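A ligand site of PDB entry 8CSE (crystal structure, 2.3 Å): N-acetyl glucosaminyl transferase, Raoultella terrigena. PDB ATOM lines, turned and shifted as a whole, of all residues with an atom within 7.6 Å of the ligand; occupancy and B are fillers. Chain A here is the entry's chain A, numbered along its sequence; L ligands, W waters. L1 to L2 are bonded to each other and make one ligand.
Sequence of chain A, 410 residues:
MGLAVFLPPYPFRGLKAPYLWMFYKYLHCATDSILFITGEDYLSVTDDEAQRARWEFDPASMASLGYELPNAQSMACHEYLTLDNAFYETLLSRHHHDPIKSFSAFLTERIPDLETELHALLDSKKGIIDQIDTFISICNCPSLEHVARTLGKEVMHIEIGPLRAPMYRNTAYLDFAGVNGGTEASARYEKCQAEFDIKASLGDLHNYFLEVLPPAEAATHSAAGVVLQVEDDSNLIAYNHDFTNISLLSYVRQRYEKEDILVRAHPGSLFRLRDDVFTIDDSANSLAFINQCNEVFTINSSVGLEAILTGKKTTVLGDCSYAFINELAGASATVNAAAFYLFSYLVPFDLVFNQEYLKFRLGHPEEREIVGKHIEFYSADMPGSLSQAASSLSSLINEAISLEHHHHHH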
ATOM      1  N   LYS A  25      26.999   6.246  28.860  1.00  0.00           N
ATOM      2  CA  LYS A  25      26.064   5.243  28.340  1.00  0.00           C
ATOM      3  C   LYS A  25      24.649   5.456  28.876  1.00  0.00           C
ATOM      4  O   LYS A  25      23.687   5.387  28.109  1.00  0.00           O
ATOM      5  CB  LYS A  25      26.582   3.833  28.669  1.00  0.00           C
ATOM      6  CG  LYS A  25      25.721   2.682  28.130  1.00  0.00           C
ATOM      7  CD  LYS A  25      25.778   2.536  26.584  1.00  0.00           C
ATOM      8  CE  LYS A  25      25.002   1.295  26.118  1.00  0.00           C
ATOM      9  NZ  LYS A  25      25.056   1.032  24.621  1.00  0.00           N
ATOM     10  N   HIS A  28      23.142   8.451  27.065  1.00  0.00           N
ATOM     11  CA  HIS A  28      22.868   8.221  25.635  1.00  0.00           C
ATOM     12  C   HIS A  28      21.557   7.456  25.493  1.00  0.00           C
ATOM     13  O   HIS A  28      20.728   7.783  24.671  1.00  0.00           O
ATOM     14  CB  HIS A  28      24.008   7.439  24.958  1.00  0.00           C
ATOM     15  CG  HIS A  28      23.883   7.354  23.455  1.00  0.00           C
ATOM     16  ND1 HIS A  28      23.743   6.164  22.783  1.00  0.00           N
ATOM     17  CD2 HIS A  28      23.883   8.324  22.507  1.00  0.00           C
ATOM     18  CE1 HIS A  28      23.670   6.397  21.476  1.00  0.00           C
ATOM     19  NE2 HIS A  28      23.739   7.696  21.285  1.00  0.00           N
ATOM     20  N   CSO A  29      21.370   6.447  26.344  1.00  0.00           N
ATOM     21  CA  CSO A  29      20.211   5.548  26.223  1.00  0.00           C
ATOM     22  CB  CSO A  29      20.569   4.132  26.754  1.00  0.00           C
ATOM     23  SG  CSO A  29      21.983   3.347  25.897  1.00  0.00           S
ATOM     24  C   CSO A  29      18.951   6.023  26.965  1.00  0.00           C
ATOM     25  O   CSO A  29      17.901   5.374  26.890  1.00  0.00           O
ATOM     26  OD  CSO A  29      21.371   2.566  24.354  1.00  0.00           O
ATOM     27  N   MET A  62      33.555   4.414  21.894  1.00  0.00           N
ATOM     28  CA  MET A  62      32.159   4.804  21.723  1.00  0.00           C
ATOM     29  C   MET A  62      31.424   3.828  20.799  1.00  0.00           C
ATOM     30  O   MET A  62      30.252   3.521  21.019  1.00  0.00           O
ATOM     31  CB  MET A  62      32.071   6.232  21.159  1.00  0.00           C
ATOM     32  CG  MET A  62      32.751   7.285  22.033  1.00  0.00           C
ATOM     33  SD  MET A  62      33.089   8.800  21.141  1.00  0.00           S
ATOM     34  CE  MET A  62      31.435   9.475  20.941  1.00  0.00           C
ATOM     35  N   ALA A  63      32.106   3.331  19.769  1.00  0.00           N
ATOM     36  CA  ALA A  63      31.438   2.381  18.894  1.00  0.00           C
ATOM     37  C   ALA A  63      31.243   1.033  19.589  1.00  0.00           C
ATOM     38  O   ALA A  63      30.173   0.433  19.466  1.00  0.00           O
ATOM     39  CB  ALA A  63      32.208   2.197  17.593  1.00  0.00           C
ATOM     40  N   SER A  64      32.245   0.563  20.329  1.00  0.00           N
ATOM     41  CA  SER A  64      32.185  -0.782  20.900  1.00  0.00           C
ATOM     42  C   SER A  64      31.166  -0.859  22.028  1.00  0.00           C
ATOM     43  O   SER A  64      30.555  -1.907  22.235  1.00  0.00           O
ATOM     44  CB  SER A  64      33.560  -1.218  21.392  1.00  0.00           C
ATOM     45  OG  SER A  64      34.372  -1.676  20.307  1.00  0.00           O
ATOM     46  N   LEU A  65      30.988   0.239  22.755  1.00  0.00           N
ATOM     47  CA  LEU A  65      30.080   0.351  23.875  1.00  0.00           C
ATOM     48  C   LEU A  65      28.744   0.967  23.508  1.00  0.00           C
ATOM     49  O   LEU A  65      27.791   0.896  24.310  1.00  0.00           O
ATOM     50  CB  LEU A  65      30.744   1.180  24.978  1.00  0.00           C
ATOM     51  CG  LEU A  65      32.164   0.751  25.324  1.00  0.00           C
ATOM     52  CD1 LEU A  65      32.669   1.486  26.560  1.00  0.00           C
ATOM     53  CD2 LEU A  65      32.184  -0.746  25.552  1.00  0.00           C
ATOM     54  N   GLY A  66      28.640   1.595  22.334  1.00  0.00           N
ATOM     55  CA  GLY A  66      27.379   2.118  21.856  1.00  0.00           C
ATOM     56  C   GLY A  66      26.866   3.370  22.552  1.00  0.00           C
ATOM     57  O   GLY A  66      25.703   3.419  22.941  1.00  0.00           O
ATOM     58  N   TYR A  67      27.713   4.383  22.738  1.00  0.00           N
ATOM     59  CA  TYR A  67      27.258   5.686  23.189  1.00  0.00           C
ATOM     60  C   TYR A  67      27.895   6.794  22.351  1.00  0.00           C
ATOM     61  O   TYR A  67      28.896   6.588  21.645  1.00  0.00           O
ATOM     62  CB  TYR A  67      27.547   5.924  24.695  1.00  0.00           C
ATOM     63  CG  TYR A  67      29.018   5.974  25.024  1.00  0.00           C
ATOM     64  CD1 TYR A  67      29.765   7.122  24.764  1.00  0.00           C
ATOM     65  CD2 TYR A  67      29.651   4.889  25.593  1.00  0.00           C
ATOM     66  CE1 TYR A  67      31.099   7.181  25.049  1.00  0.00           C
ATOM     67  CE2 TYR A  67      31.011   4.939  25.890  1.00  0.00           C
ATOM     68  CZ  TYR A  67      31.719   6.098  25.624  1.00  0.00           C
ATOM     69  OH  TYR A  67      33.066   6.173  25.918  1.00  0.00           O
ATOM     70  N   GLU A  68      27.290   7.972  22.428  1.00  0.00           N
ATOM     71  CA  GLU A  68      27.832   9.212  21.901  1.00  0.00           C
ATOM     72  C   GLU A  68      28.152  10.130  23.072  1.00  0.00           C
ATOM     73  O   GLU A  68      27.528  10.057  24.137  1.00  0.00           O
ATOM     74  CB  GLU A  68      26.826   9.887  20.940  1.00  0.00           C
ATOM     75  CG  GLU A  68      26.829   9.238  19.552  1.00  0.00           C
ATOM     76  CD  GLU A  68      25.637   9.637  18.673  1.00  0.00           C
ATOM     77  OE1 GLU A  68      24.843  10.544  19.022  1.00  0.00           O
ATOM     78  OE2 GLU A  68      25.494   9.004  17.598  1.00  0.00           O
ATOM     79  N   ALA A 165      32.959  -7.184  23.545  1.00  0.00           N
ATOM     80  CA  ALA A 165      33.385  -6.997  22.162  1.00  0.00           C
ATOM     81  C   ALA A 165      34.865  -6.609  22.107  1.00  0.00           C
ATOM     82  O   ALA A 165      35.403  -6.043  23.065  1.00  0.00           O
ATOM     83  CB  ALA A 165      32.527  -5.933  21.490  1.00  0.00           C
ATOM     84  N   PRO A 166      35.550  -6.897  20.997  1.00  0.00           N
ATOM     85  CA  PRO A 166      35.013  -7.502  19.775  1.00  0.00           C
ATOM     86  C   PRO A 166      34.921  -9.017  19.754  1.00  0.00           C
ATOM     87  O   PRO A 166      34.253  -9.558  18.849  1.00  0.00           O
ATOM     88  CB  PRO A 166      36.004  -7.063  18.698  1.00  0.00           C
ATOM     89  CG  PRO A 166      37.283  -6.820  19.423  1.00  0.00           C
ATOM     90  CD  PRO A 166      36.980  -6.558  20.887  1.00  0.00           C
ATOM     91  N   TYR A 168      33.381 -11.056  21.618  1.00  0.00           N
ATOM     92  CA  TYR A 168      32.113 -11.587  22.094  1.00  0.00           C
ATOM     93  C   TYR A 168      31.010 -10.533  21.963  1.00  0.00           C
ATOM     94  O   TYR A 168      31.274  -9.334  21.877  1.00  0.00           O
ATOM     95  CB  TYR A 168      32.237 -12.031  23.564  1.00  0.00           C
ATOM     96  CG  TYR A 168      33.307 -13.068  23.782  1.00  0.00           C
ATOM     97  CD1 TYR A 168      33.072 -14.398  23.447  1.00  0.00           C
ATOM     98  CD2 TYR A 168      34.553 -12.736  24.312  1.00  0.00           C
ATOM     99  CE1 TYR A 168      34.025 -15.371  23.639  1.00  0.00           C
ATOM    100  CE2 TYR A 168      35.530 -13.728  24.513  1.00  0.00           C
ATOM    101  CZ  TYR A 168      35.248 -15.044  24.168  1.00  0.00           C
ATOM    102  OH  TYR A 168      36.164 -16.057  24.336  1.00  0.00           O
ATOM    103  N   ARG A 169      29.768 -11.019  21.952  1.00  0.00           N
ATOM    104  CA  ARG A 169      28.643 -10.141  22.280  1.00  0.00           C
ATOM    105  C   ARG A 169      28.910  -9.474  23.613  1.00  0.00           C
ATOM    106  O   ARG A 169      29.334 -10.117  24.572  1.00  0.00           O
ATOM    107  CB  ARG A 169      27.349 -10.932  22.390  1.00  0.00           C
ATOM    108  CG  ARG A 169      27.117 -12.063  21.400  1.00  0.00           C
ATOM    109  CD  ARG A 169      25.725 -12.697  21.642  1.00  0.00           C
ATOM    110  NE  ARG A 169      25.478 -13.847  20.776  1.00  0.00           N
ATOM    111  CZ  ARG A 169      24.547 -13.903  19.847  1.00  0.00           C
ATOM    112  NH1 ARG A 169      23.724 -12.886  19.624  1.00  0.00           N
ATOM    113  NH2 ARG A 169      24.404 -15.027  19.126  1.00  0.00           N
ATOM    114  N   ASN A 170      28.605  -8.174  23.699  1.00  0.00           N
ATOM    115  CA  ASN A 170      28.761  -7.478  24.971  1.00  0.00           C
ATOM    116  C   ASN A 170      27.780  -7.996  26.018  1.00  0.00           C
ATOM    117  O   ASN A 170      26.583  -8.150  25.741  1.00  0.00           O
ATOM    118  CB  ASN A 170      28.623  -5.979  24.752  1.00  0.00           C
ATOM    119  CG  ASN A 170      29.895  -5.389  24.208  1.00  0.00           C
ATOM    120  OD1 ASN A 170      30.999  -5.757  24.666  1.00  0.00           O
ATOM    121  ND2 ASN A 170      29.783  -4.504  23.192  1.00  0.00           N
ATOM    122  N   THR A 171      28.275  -8.281  27.211  1.00  0.00           N
ATOM    123  CA  THR A 171      27.445  -8.702  28.325  1.00  0.00           C
ATOM    124  C   THR A 171      27.579  -7.708  29.483  1.00  0.00           C
ATOM    125  O   THR A 171      28.508  -6.904  29.510  1.00  0.00           O
ATOM    126  CB  THR A 171      27.787 -10.136  28.778  1.00  0.00           C
ATOM    127  OG1 THR A 171      29.183 -10.213  29.130  1.00  0.00           O
ATOM    128  CG2 THR A 171      27.472 -11.122  27.621  1.00  0.00           C
ATOM    129  N   GLU A 211      31.748 -13.725  18.549  1.00  0.00           N
ATOM    130  CA  GLU A 211      31.424 -12.906  17.395  1.00  0.00           C
ATOM    131  C   GLU A 211      32.452 -13.017  16.289  1.00  0.00           C
ATOM    132  O   GLU A 211      32.241 -12.460  15.198  1.00  0.00           O
ATOM    133  CB  GLU A 211      31.294 -11.438  17.829  1.00  0.00           C
ATOM    134  CG  GLU A 211      30.090 -11.127  18.709  1.00  0.00           C
ATOM    135  CD  GLU A 211      28.823 -11.044  17.892  1.00  0.00           C
ATOM    136  OE1 GLU A 211      28.361 -12.109  17.417  1.00  0.00           O
ATOM    137  OE2 GLU A 211      28.304  -9.915  17.713  1.00  0.00           O
ATOM    138  N   PRO A 348      22.311  -9.110  28.226  1.00  0.00           N
ATOM    139  CA  PRO A 348      22.725  -8.393  27.006  1.00  0.00           C
ATOM    140  C   PRO A 348      23.109  -6.969  27.383  1.00  0.00           C
ATOM    141  O   PRO A 348      22.319  -6.248  27.999  1.00  0.00           O
ATOM    142  CB  PRO A 348      21.484  -8.434  26.116  1.00  0.00           C
ATOM    143  CG  PRO A 348      20.791  -9.682  26.512  1.00  0.00           C
ATOM    144  CD  PRO A 348      21.064  -9.881  28.013  1.00  0.00           C
ATOM    145  N   PHE A 349      24.330  -6.563  27.023  1.00  0.00           N
ATOM    146  CA  PHE A 349      24.903  -5.321  27.534  1.00  0.00           C
ATOM    147  C   PHE A 349      23.906  -4.152  27.484  1.00  0.00           C
ATOM    148  O   PHE A 349      23.686  -3.464  28.489  1.00  0.00           O
ATOM    149  CB  PHE A 349      26.171  -4.987  26.759  1.00  0.00           C
ATOM    150  CG  PHE A 349      26.907  -3.741  27.239  1.00  0.00           C
ATOM    151  CD1 PHE A 349      27.703  -3.773  28.381  1.00  0.00           C
ATOM    152  CD2 PHE A 349      26.834  -2.558  26.511  1.00  0.00           C
ATOM    153  CE1 PHE A 349      28.401  -2.627  28.794  1.00  0.00           C
ATOM    154  CE2 PHE A 349      27.522  -1.419  26.918  1.00  0.00           C
ATOM    155  CZ  PHE A 349      28.298  -1.455  28.050  1.00  0.00           C
ATOM    156  N   ASP A 350      23.304  -3.904  26.323  1.00  0.00           N
ATOM    157  CA  ASP A 350      22.462  -2.718  26.194  1.00  0.00           C
ATOM    158  C   ASP A 350      21.281  -2.739  27.160  1.00  0.00           C
ATOM    159  O   ASP A 350      20.811  -1.681  27.590  1.00  0.00           O
ATOM    160  CB  ASP A 350      21.978  -2.602  24.746  1.00  0.00           C
ATOM    161  CG  ASP A 350      23.039  -2.018  23.826  1.00  0.00           C
ATOM    162  OD1 ASP A 350      24.032  -1.498  24.371  1.00  0.00           O
ATOM    163  OD2 ASP A 350      22.886  -2.079  22.583  1.00  0.00           O
ATOM    164  N   LEU A 351      20.795  -3.916  27.557  1.00  0.00           N
ATOM    165  CA  LEU A 351      19.561  -3.949  28.326  1.00  0.00           C
ATOM    166  C   LEU A 351      19.726  -3.329  29.725  1.00  0.00           C
ATOM    167  O   LEU A 351      18.738  -2.872  30.306  1.00  0.00           O
ATOM    168  CB  LEU A 351      19.031  -5.373  28.405  1.00  0.00           C
ATOM    169  CG  LEU A 351      18.437  -5.951  27.126  1.00  0.00           C
ATOM    170  CD1 LEU A 351      17.939  -7.347  27.360  1.00  0.00           C
ATOM    171  CD2 LEU A 351      17.321  -5.077  26.636  1.00  0.00           C
ATOM    172  N   PHE A 353      20.990  -0.602  30.482  1.00  0.00           N
ATOM    173  CA  PHE A 353      20.810   0.835  30.336  1.00  0.00           C
ATOM    174  C   PHE A 353      19.457   1.133  29.744  1.00  0.00           C
ATOM    175  O   PHE A 353      19.159   2.288  29.397  1.00  0.00           O
ATOM    176  CB  PHE A 353      21.951   1.397  29.475  1.00  0.00           C
ATOM    177  CG  PHE A 353      23.323   0.931  29.926  1.00  0.00           C
ATOM    178  CD1 PHE A 353      24.006   1.613  30.928  1.00  0.00           C
ATOM    179  CD2 PHE A 353      23.904  -0.227  29.379  1.00  0.00           C
ATOM    180  CE1 PHE A 353      25.279   1.187  31.348  1.00  0.00           C
ATOM    181  CE2 PHE A 353      25.164  -0.674  29.812  1.00  0.00           C
ATOM    182  CZ  PHE A 353      25.843   0.035  30.792  1.00  0.00           C
ATOM    183  N   PHE A 377      16.539 -10.636  22.717  1.00  0.00           N
ATOM    184  CA  PHE A 377      17.524  -9.633  22.328  1.00  0.00           C
ATOM    185  C   PHE A 377      18.588 -10.248  21.435  1.00  0.00           C
ATOM    186  O   PHE A 377      18.851  -9.761  20.332  1.00  0.00           O
ATOM    187  CB  PHE A 377      18.151  -9.001  23.575  1.00  0.00           C
ATOM    188  CG  PHE A 377      19.042  -7.829  23.266  1.00  0.00           C
ATOM    189  CD1 PHE A 377      20.371  -8.019  22.916  1.00  0.00           C
ATOM    190  CD2 PHE A 377      18.536  -6.533  23.286  1.00  0.00           C
ATOM    191  CE1 PHE A 377      21.180  -6.938  22.620  1.00  0.00           C
ATOM    192  CE2 PHE A 377      19.342  -5.471  22.986  1.00  0.00           C
ATOM    193  CZ  PHE A 377      20.664  -5.677  22.664  1.00  0.00           C
HETATM  194  C1  LIG L   1      28.168  -2.635  19.350  1.00  0.00           C
HETATM  195  C2  LIG L   1      26.912  -2.276  18.558  1.00  0.00           C
HETATM  196  C3  LIG L   1      26.089  -1.239  19.328  1.00  0.00           C
HETATM  197  C4  LIG L   1      25.856  -1.661  20.770  1.00  0.00           C
HETATM  198  C5  LIG L   1      27.150  -2.135  21.441  1.00  0.00           C
HETATM  199  C6  LIG L   1      26.905  -2.812  22.773  1.00  0.00           C
HETATM  200  C7  LIG L   1      26.511  -1.996  16.150  1.00  0.00           C
HETATM  201  C8  LIG L   1      27.023  -1.411  14.869  1.00  0.00           C
HETATM  202  N1  LIG L   1      27.254  -1.781  17.235  1.00  0.00           N
HETATM  203  O1  LIG L   1      28.883  -3.650  18.710  1.00  0.00           O
HETATM  204  O2  LIG L   1      24.824  -1.144  18.671  1.00  0.00           O
HETATM  205  O3  LIG L   1      25.277  -0.585  21.510  1.00  0.00           O
HETATM  206  O4  LIG L   1      27.805  -3.109  20.608  1.00  0.00           O
HETATM  207  O5  LIG L   1      26.423  -4.136  22.587  1.00  0.00           O
HETATM  208  O6  LIG L   1      25.466  -2.644  16.191  1.00  0.00           O
HETATM  209  C1  LG2 L   2      24.483   0.086  17.987  1.00  0.00           C
HETATM  210  C2  LG2 L   2      23.182  -0.285  17.244  1.00  0.00           C
HETATM  211  C3  LG2 L   2      22.010  -0.322  18.178  1.00  0.00           C
HETATM  212  C4  LG2 L   2      21.972   0.943  18.999  1.00  0.00           C
HETATM  213  C5  LG2 L   2      23.246   1.210  19.803  1.00  0.00           C
HETATM  214  C6  LG2 L   2      23.289   2.509  20.545  1.00  0.00           C
HETATM  215  O1  LG2 L   2      22.925   0.645  16.174  1.00  0.00           O
HETATM  216  O2  LG2 L   2      20.751  -0.436  17.427  1.00  0.00           O
HETATM  217  O3  LG2 L   2      20.914   0.898  19.955  1.00  0.00           O
HETATM  218  O4  LG2 L   2      24.409   1.256  18.922  1.00  0.00           O
HETATM  219  O   HOH W   1      27.338  -6.973  21.146  1.00  0.00           O
HETATM  220  O   HOH W   2      24.158  -5.298  23.906  1.00  0.00           O
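The side-chain carboxylate of Asp 350 lies within hydrogen-bond range of an oxygen (O3) of LIG L1, at 3.0 Å.
The side-chain amide nitrogen (ND2) of Asn 170 sits close to an oxygen (O5) of LIG L1 (3.4 Å).
ND2 of Asn 170 sits at hydrogen-bond distance from O of Ser 64, 2.9 Å away.
NZ of Lys 25 lies within hydrogen-bond range of O of Leu 65 (2.8 Å).
OD1 of Asn 170 sits at hydrogen-bond distance from N of Ala 165.
O of Gly 66 lies within hydrogen-bond range of ND1 of His 28, at 3.4 Å.
The backbone carbonyl oxygen (O) of Gly 66 lies within hydrogen-bond range of the side-chain amino group (NZ) of Lys 25 (3.0 Å).
The backbone carbonyl oxygen (O) of Asn 170 lies within hydrogen-bond range of the backbone NH (N) of Phe 349 (3.0 Å).
The side-chain amino group of Lys 25 lies within salt-bridge range of the side-chain carboxylate of Asp 350, 2.7 Å away.
The backbone carbonyl oxygen (O) of Ser 64 sits close to an oxygen (O4) of LIG L1.
Residues that only touch the ligand: Gly 66 (3.4 Å), Lys 25 (3.5 Å), Ala 63 (3.7 Å) and Phe 349 (3.7 Å).
Hydrophobic or aromatic side chains that line the ligand: Phe 349.
Along chain A the residues within 4 Å of the ligand span positions 25 to 350.
Water W2 lies within hydrogen-bond range of O5 of LIG L1, N of Asp 350 and N of Phe 349.
Water W1 lies within hydrogen-bond range of the backbone NH (N) of Asn 170 (3.1 Å) and an oxygen (O5) of LIG L1 (3.3 Å).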
